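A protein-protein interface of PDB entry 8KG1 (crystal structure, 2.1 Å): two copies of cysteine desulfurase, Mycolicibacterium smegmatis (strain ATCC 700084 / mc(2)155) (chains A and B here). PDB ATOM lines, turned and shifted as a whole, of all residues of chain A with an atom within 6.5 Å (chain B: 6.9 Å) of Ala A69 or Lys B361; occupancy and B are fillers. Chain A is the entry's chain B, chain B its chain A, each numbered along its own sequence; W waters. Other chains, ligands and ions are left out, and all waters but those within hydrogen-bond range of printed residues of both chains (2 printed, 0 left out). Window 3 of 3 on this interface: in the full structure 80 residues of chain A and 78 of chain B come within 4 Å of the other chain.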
ATOM      1  N   HIS A  67     -14.808  28.403 -35.402  1.00  0.00           N
ATOM      2  CA  HIS A  67     -15.170  28.072 -34.019  1.00  0.00           C
ATOM      3  C   HIS A  67     -13.922  28.062 -33.144  1.00  0.00           C
ATOM      4  O   HIS A  67     -13.265  27.028 -32.983  1.00  0.00           O
ATOM      5  CB  HIS A  67     -15.935  26.749 -33.907  1.00  0.00           C
ATOM      6  CG  HIS A  67     -17.364  26.850 -34.338  1.00  0.00           C
ATOM      7  ND1 HIS A  67     -17.734  27.352 -35.569  1.00  0.00           N
ATOM      8  CD2 HIS A  67     -18.514  26.526 -33.703  1.00  0.00           C
ATOM      9  CE1 HIS A  67     -19.050  27.327 -35.674  1.00  0.00           C
ATOM     10  NE2 HIS A  67     -19.548  26.828 -34.557  1.00  0.00           N
ATOM     11  N   ARG A  68     -13.601  29.219 -32.561  1.00  0.00           N
ATOM     12  CA  ARG A  68     -12.299  29.419 -31.933  1.00  0.00           C
ATOM     13  C   ARG A  68     -12.086  28.562 -30.688  1.00  0.00           C
ATOM     14  O   ARG A  68     -10.932  28.336 -30.303  1.00  0.00           O
ATOM     15  CB  ARG A  68     -12.110  30.903 -31.590  1.00  0.00           C
ATOM     16  CG  ARG A  68     -13.178  31.468 -30.678  1.00  0.00           C
ATOM     17  CD  ARG A  68     -12.789  32.846 -30.180  1.00  0.00           C
ATOM     18  NE  ARG A  68     -13.127  33.878 -31.151  1.00  0.00           N
ATOM     19  CZ  ARG A  68     -12.230  34.532 -31.872  1.00  0.00           C
ATOM     20  NH1 ARG A  68     -10.938  34.258 -31.772  1.00  0.00           N
ATOM     21  NH2 ARG A  68     -12.637  35.482 -32.718  1.00  0.00           N
ATOM     22  N   ALA A  69     -13.153  28.077 -30.049  1.00  0.00           N
ATOM     23  CA  ALA A  69     -12.956  27.207 -28.894  1.00  0.00           C
ATOM     24  C   ALA A  69     -12.361  25.851 -29.270  1.00  0.00           C
ATOM     25  O   ALA A  69     -11.849  25.152 -28.387  1.00  0.00           O
ATOM     26  CB  ALA A  69     -14.284  27.001 -28.152  1.00  0.00           C
ATOM     27  N   ALA A  70     -12.414  25.462 -30.549  1.00  0.00           N
ATOM     28  CA  ALA A  70     -12.003  24.115 -30.944  1.00  0.00           C
ATOM     29  C   ALA A  70     -10.495  23.919 -30.787  1.00  0.00           C
ATOM     30  O   ALA A  70     -10.046  23.007 -30.081  1.00  0.00           O
ATOM     31  CB  ALA A  70     -12.435  23.836 -32.389  1.00  0.00           C
ATOM     32  N   HIS A  71      -9.696  24.756 -31.440  1.00  0.00           N
ATOM     33  CA  HIS A  71      -8.243  24.608 -31.398  1.00  0.00           C
ATOM     34  C   HIS A  71      -7.603  25.854 -32.009  1.00  0.00           C
ATOM     35  O   HIS A  71      -8.288  26.769 -32.480  1.00  0.00           O
ATOM     36  CB  HIS A  71      -7.787  23.322 -32.105  1.00  0.00           C
ATOM     37  CG  HIS A  71      -8.396  23.106 -33.461  1.00  0.00           C
ATOM     38  ND1 HIS A  71      -8.077  23.884 -34.556  1.00  0.00           N
ATOM     39  CD2 HIS A  71      -9.290  22.187 -33.904  1.00  0.00           C
ATOM     40  CE1 HIS A  71      -8.746  23.454 -35.612  1.00  0.00           C
ATOM     41  NE2 HIS A  71      -9.490  22.424 -35.247  1.00  0.00           N
ATOM     42  N   ALA A  74      -8.275  26.840 -35.666  1.00  0.00           N
ATOM     43  CA  ALA A  74      -9.671  27.260 -35.756  1.00  0.00           C
ATOM     44  C   ALA A  74      -9.850  28.676 -35.222  1.00  0.00           C
ATOM     45  O   ALA A  74     -10.622  29.461 -35.780  1.00  0.00           O
ATOM     46  CB  ALA A  74     -10.583  26.280 -35.008  1.00  0.00           C
ATOM     47  N   ALA A  75      -9.101  29.037 -34.170  1.00  0.00           N
ATOM     48  CA  ALA A  75      -9.186  30.388 -33.617  1.00  0.00           C
ATOM     49  C   ALA A  75      -8.579  31.421 -34.565  1.00  0.00           C
ATOM     50  O   ALA A  75      -9.133  32.513 -34.735  1.00  0.00           O
ATOM     51  CB  ALA A  75      -8.499  30.450 -32.252  1.00  0.00           C
ATOM     52  N   THR A  78     -11.136  31.867 -37.307  1.00  0.00           N
ATOM     53  CA  THR A  78     -12.277  32.647 -36.836  1.00  0.00           C
ATOM     54  C   THR A  78     -11.932  34.125 -36.740  1.00  0.00           C
ATOM     55  O   THR A  78     -12.720  34.980 -37.163  1.00  0.00           O
ATOM     56  CB  THR A  78     -12.760  32.127 -35.488  1.00  0.00           C
ATOM     57  OG1 THR A  78     -13.060  30.733 -35.606  1.00  0.00           O
ATOM     58  CG2 THR A  78     -14.019  32.878 -35.045  1.00  0.00           C
ATOM     59  N   PRO B 356     -16.547  15.900 -23.666  1.00  0.00           N
ATOM     60  CA  PRO B 356     -15.791  15.908 -24.935  1.00  0.00           C
ATOM     61  C   PRO B 356     -15.050  17.204 -25.216  1.00  0.00           C
ATOM     62  O   PRO B 356     -13.895  17.169 -25.661  1.00  0.00           O
ATOM     63  CB  PRO B 356     -16.885  15.659 -25.977  1.00  0.00           C
ATOM     64  CG  PRO B 356     -17.865  14.779 -25.261  1.00  0.00           C
ATOM     65  CD  PRO B 356     -17.858  15.241 -23.809  1.00  0.00           C
ATOM     66  N   LEU B 357     -15.680  18.354 -24.966  1.00  0.00           N
ATOM     67  CA  LEU B 357     -15.038  19.627 -25.292  1.00  0.00           C
ATOM     68  C   LEU B 357     -13.791  19.869 -24.436  1.00  0.00           C
ATOM     69  O   LEU B 357     -12.794  20.421 -24.919  1.00  0.00           O
ATOM     70  CB  LEU B 357     -16.047  20.766 -25.132  1.00  0.00           C
ATOM     71  CG  LEU B 357     -15.555  22.203 -25.344  1.00  0.00           C
ATOM     72  CD1 LEU B 357     -14.821  22.387 -26.687  1.00  0.00           C
ATOM     73  CD2 LEU B 357     -16.722  23.166 -25.219  1.00  0.00           C
ATOM     74  N   GLU B 358     -13.811  19.455 -23.165  1.00  0.00           N
ATOM     75  CA  GLU B 358     -12.609  19.626 -22.355  1.00  0.00           C
ATOM     76  C   GLU B 358     -11.483  18.709 -22.824  1.00  0.00           C
ATOM     77  O   GLU B 358     -10.304  19.086 -22.756  1.00  0.00           O
ATOM     78  CB  GLU B 358     -12.924  19.400 -20.875  1.00  0.00           C
ATOM     79  CG  GLU B 358     -13.775  20.530 -20.257  1.00  0.00           C
ATOM     80  CD  GLU B 358     -13.272  21.941 -20.625  1.00  0.00           C
ATOM     81  OE1 GLU B 358     -12.131  22.306 -20.227  1.00  0.00           O
ATOM     82  OE2 GLU B 358     -14.020  22.680 -21.323  1.00  0.00           O
ATOM     83  N   VAL B 359     -11.818  17.516 -23.317  1.00  0.00           N
ATOM     84  CA  VAL B 359     -10.790  16.659 -23.903  1.00  0.00           C
ATOM     85  C   VAL B 359     -10.204  17.319 -25.146  1.00  0.00           C
ATOM     86  O   VAL B 359      -8.984  17.313 -25.357  1.00  0.00           O
ATOM     87  CB  VAL B 359     -11.369  15.266 -24.214  1.00  0.00           C
ATOM     88  CG1 VAL B 359     -10.316  14.375 -24.895  1.00  0.00           C
ATOM     89  CG2 VAL B 359     -11.919  14.623 -22.938  1.00  0.00           C
ATOM     90  N   GLY B 360     -11.063  17.899 -25.990  1.00  0.00           N
ATOM     91  CA  GLY B 360     -10.562  18.584 -27.176  1.00  0.00           C
ATOM     92  C   GLY B 360      -9.634  19.736 -26.828  1.00  0.00           C
ATOM     93  O   GLY B 360      -8.599  19.938 -27.473  1.00  0.00           O
ATOM     94  N   LYS B 361      -9.976  20.492 -25.782  1.00  0.00           N
ATOM     95  CA  LYS B 361      -9.129  21.621 -25.406  1.00  0.00           C
ATOM     96  C   LYS B 361      -7.818  21.160 -24.785  1.00  0.00           C
ATOM     97  O   LYS B 361      -6.768  21.773 -25.014  1.00  0.00           O
ATOM     98  CB  LYS B 361      -9.878  22.551 -24.457  1.00  0.00           C
ATOM     99  CG  LYS B 361     -11.098  23.177 -25.100  1.00  0.00           C
ATOM    100  CD  LYS B 361     -11.173  24.662 -24.815  1.00  0.00           C
ATOM    101  CE  LYS B 361     -12.355  24.964 -23.937  1.00  0.00           C
ATOM    102  NZ  LYS B 361     -13.613  24.851 -24.701  1.00  0.00           N
ATOM    103  N   ALA B 362      -7.843  20.074 -24.008  1.00  0.00           N
ATOM    104  CA  ALA B 362      -6.585  19.547 -23.484  1.00  0.00           C
ATOM    105  C   ALA B 362      -5.697  19.032 -24.614  1.00  0.00           C
ATOM    106  O   ALA B 362      -4.467  19.241 -24.610  1.00  0.00           O
ATOM    107  CB  ALA B 362      -6.866  18.440 -22.470  1.00  0.00           C
ATOM    108  N   LEU B 363      -6.309  18.378 -25.605  1.00  0.00           N
ATOM    109  CA  LEU B 363      -5.541  17.903 -26.751  1.00  0.00           C
ATOM    110  C   LEU B 363      -4.925  19.073 -27.502  1.00  0.00           C
ATOM    111  O   LEU B 363      -3.760  19.007 -27.907  1.00  0.00           O
ATOM    112  CB  LEU B 363      -6.424  17.060 -27.679  1.00  0.00           C
ATOM    113  CG  LEU B 363      -6.816  15.714 -27.042  1.00  0.00           C
ATOM    114  CD1 LEU B 363      -7.718  14.885 -27.963  1.00  0.00           C
ATOM    115  CD2 LEU B 363      -5.585  14.921 -26.620  1.00  0.00           C
ATOM    116  N   ASN B 364      -5.681  20.168 -27.662  1.00  0.00           N
ATOM    117  CA  ASN B 364      -5.119  21.350 -28.314  1.00  0.00           C
ATOM    118  C   ASN B 364      -3.955  21.907 -27.514  1.00  0.00           C
ATOM    119  O   ASN B 364      -2.974  22.393 -28.091  1.00  0.00           O
ATOM    120  CB  ASN B 364      -6.175  22.436 -28.507  1.00  0.00           C
ATOM    121  CG  ASN B 364      -5.583  23.721 -29.090  1.00  0.00           C
ATOM    122  OD1 ASN B 364      -5.098  23.740 -30.228  1.00  0.00           O
ATOM    123  ND2 ASN B 364      -5.590  24.790 -28.297  1.00  0.00           N
ATOM    124  N   ALA B 365      -4.046  21.853 -26.178  1.00  0.00           N
ATOM    125  CA  ALA B 365      -2.904  22.251 -25.358  1.00  0.00           C
ATOM    126  C   ALA B 365      -1.678  21.403 -25.669  1.00  0.00           C
ATOM    127  O   ALA B 365      -0.542  21.860 -25.477  1.00  0.00           O
ATOM    128  CB  ALA B 365      -3.246  22.159 -23.867  1.00  0.00           C
ATOM    129  N   GLU B 366      -1.879  20.168 -26.128  1.00  0.00           N
ATOM    130  CA  GLU B 366      -0.752  19.354 -26.595  1.00  0.00           C
ATOM    131  C   GLU B 366      -0.385  19.602 -28.068  1.00  0.00           C
ATOM    132  O   GLU B 366       0.453  18.879 -28.619  1.00  0.00           O
ATOM    133  CB  GLU B 366      -1.054  17.867 -26.406  1.00  0.00           C
ATOM    134  CG  GLU B 366      -1.209  17.434 -24.973  1.00  0.00           C
ATOM    135  CD  GLU B 366       0.044  17.682 -24.188  1.00  0.00           C
ATOM    136  OE1 GLU B 366       0.000  18.532 -23.271  1.00  0.00           O
ATOM    137  OE2 GLU B 366       1.085  17.071 -24.525  1.00  0.00           O
ATOM    138  N   ILE B 368      -2.552  19.127 -30.525  1.00  0.00           N
ATOM    139  CA  ILE B 368      -3.373  18.241 -31.343  1.00  0.00           C
ATOM    140  C   ILE B 368      -4.701  18.920 -31.646  1.00  0.00           C
ATOM    141  O   ILE B 368      -5.434  19.299 -30.730  1.00  0.00           O
ATOM    142  CB  ILE B 368      -3.607  16.895 -30.631  1.00  0.00           C
ATOM    143  CG1 ILE B 368      -2.276  16.180 -30.354  1.00  0.00           C
ATOM    144  CG2 ILE B 368      -4.560  16.025 -31.448  1.00  0.00           C
ATOM    145  CD1 ILE B 368      -2.296  15.272 -29.116  1.00  0.00           C
ATOM    146  N   VAL B 370      -8.415  18.496 -32.872  1.00  0.00           N
ATOM    147  CA  VAL B 370      -9.562  17.622 -33.087  1.00  0.00           C
ATOM    148  C   VAL B 370     -10.819  18.459 -32.875  1.00  0.00           C
ATOM    149  O   VAL B 370     -10.767  19.572 -32.351  1.00  0.00           O
ATOM    150  CB  VAL B 370      -9.580  16.404 -32.138  1.00  0.00           C
ATOM    151  CG1 VAL B 370      -8.286  15.622 -32.210  1.00  0.00           C
ATOM    152  CG2 VAL B 370      -9.833  16.873 -30.700  1.00  0.00           C
ATOM    153  N   ARG B 371     -11.963  17.923 -33.288  1.00  0.00           N
ATOM    154  CA  ARG B 371     -13.244  18.531 -32.957  1.00  0.00           C
ATOM    155  C   ARG B 371     -13.922  17.704 -31.885  1.00  0.00           C
ATOM    156  O   ARG B 371     -13.920  16.471 -31.942  1.00  0.00           O
ATOM    157  CB  ARG B 371     -14.182  18.630 -34.162  1.00  0.00           C
ATOM    158  CG  ARG B 371     -13.720  19.559 -35.239  1.00  0.00           C
ATOM    159  CD  ARG B 371     -14.090  21.004 -35.023  1.00  0.00           C
ATOM    160  NE  ARG B 371     -13.358  21.831 -35.977  1.00  0.00           N
ATOM    161  CZ  ARG B 371     -13.551  23.131 -36.142  1.00  0.00           C
ATOM    162  NH1 ARG B 371     -14.489  23.780 -35.472  1.00  0.00           N
ATOM    163  NH2 ARG B 371     -12.792  23.792 -37.007  1.00  0.00           N
ATOM    164  N   ALA B 372     -14.517  18.393 -30.922  1.00  0.00           N
ATOM    165  CA  ALA B 372     -15.372  17.779 -29.924  1.00  0.00           C
ATOM    166  C   ALA B 372     -16.724  18.460 -30.040  1.00  0.00           C
ATOM    167  O   ALA B 372     -16.809  19.691 -29.948  1.00  0.00           O
ATOM    168  CB  ALA B 372     -14.789  17.935 -28.518  1.00  0.00           C
ATOM    169  N   ILE B 413      -5.002  12.331 -19.736  1.00  0.00           N
ATOM    170  CA  ILE B 413      -6.291  12.895 -19.342  1.00  0.00           C
ATOM    171  C   ILE B 413      -7.094  11.877 -18.539  1.00  0.00           C
ATOM    172  O   ILE B 413      -7.707  12.213 -17.516  1.00  0.00           O
ATOM    173  CB  ILE B 413      -7.069  13.390 -20.575  1.00  0.00           C
ATOM    174  CG1 ILE B 413      -6.361  14.586 -21.224  1.00  0.00           C
ATOM    175  CG2 ILE B 413      -8.494  13.763 -20.196  1.00  0.00           C
ATOM    176  CD1 ILE B 413      -6.796  14.834 -22.679  1.00  0.00           C
HETATM  177  O   HOH W   1     -11.341  20.846 -29.632  1.00  0.00           O
HETATM  178  O   HOH W   2      -8.980  25.149 -27.720  1.00  0.00           O
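The backbone NH (N) of His A67 is in hydrogen-bond range of the side-chain hydroxyl (OG1) of Thr A78 (2.9 Å).
The backbone NH (N) of Ala A74 lies within hydrogen-bond range of a ring nitrogen (ND1) of His A71, at 3.2 Å.
The backbone carbonyl oxygen of Ala A74 is in hydrogen-bond range of the side-chain hydroxyl of Thr A78, 2.8 Å away.
His A67 touches Arg B371 (CB to NH1, 3.7 Å).
Ala A69 touches Lys B361.
Arg B371 touches Ala A70 (NH1 to CB, 3.7 Å).
Asn B364 touches His A71.
Val B370 touches His A71.
His A71 touches Arg B371.
Ala A74 touches Arg B371 (CB to NH2, 3.9 Å).
Ala A69 touches one residue of chain B.
Of chain A, only Ala A69 (3.7 Å) comes within 4 Å of Lys B361.
Of the printed residues of chain A, Asn B364 touches His A71 (3.3 Å).
Printed residues of chain A within 4 Å of Arg B371: His A67 (3.7 Å), Ala A70 (3.7 Å), His A71 (3.98 Å) and Ala A74 (3.9 Å).
Of the printed residues of chain B, His A71 touches Asn B364 (3.3 Å), Val B370 (3.4 Å) and Arg B371 (3.98 Å).
Printed residues of chain A within 4 Å of Val B370: His A71 (3.4 Å).
Printed residues of chain B within 4 Å of Ala A70: Arg B371.
The nearest printed residue of chain B that does not touch Ala A74 is Asn B364 (7.0 Å).
Hydrophobic or aromatic side chains of chain A within 4 Å of the printed part of chain B: His A67, Ala A70, His A71 and Ala A74.
Along chain A the printed residues that touch a printed residue of chain B span positions 67 to 74.
No position is printed for both chains.
Water W1 lies within hydrogen-bond range of O of Ala A70 (2.6 Å) and O of Val B370 (3.1 Å).
Water W2 lies within hydrogen-bond range of the backbone carbonyl oxygen (O) of Ala A69, the backbone carbonyl oxygen (O) of Ala A70 and the side-chain amide nitrogen (ND2) of Asn B364.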
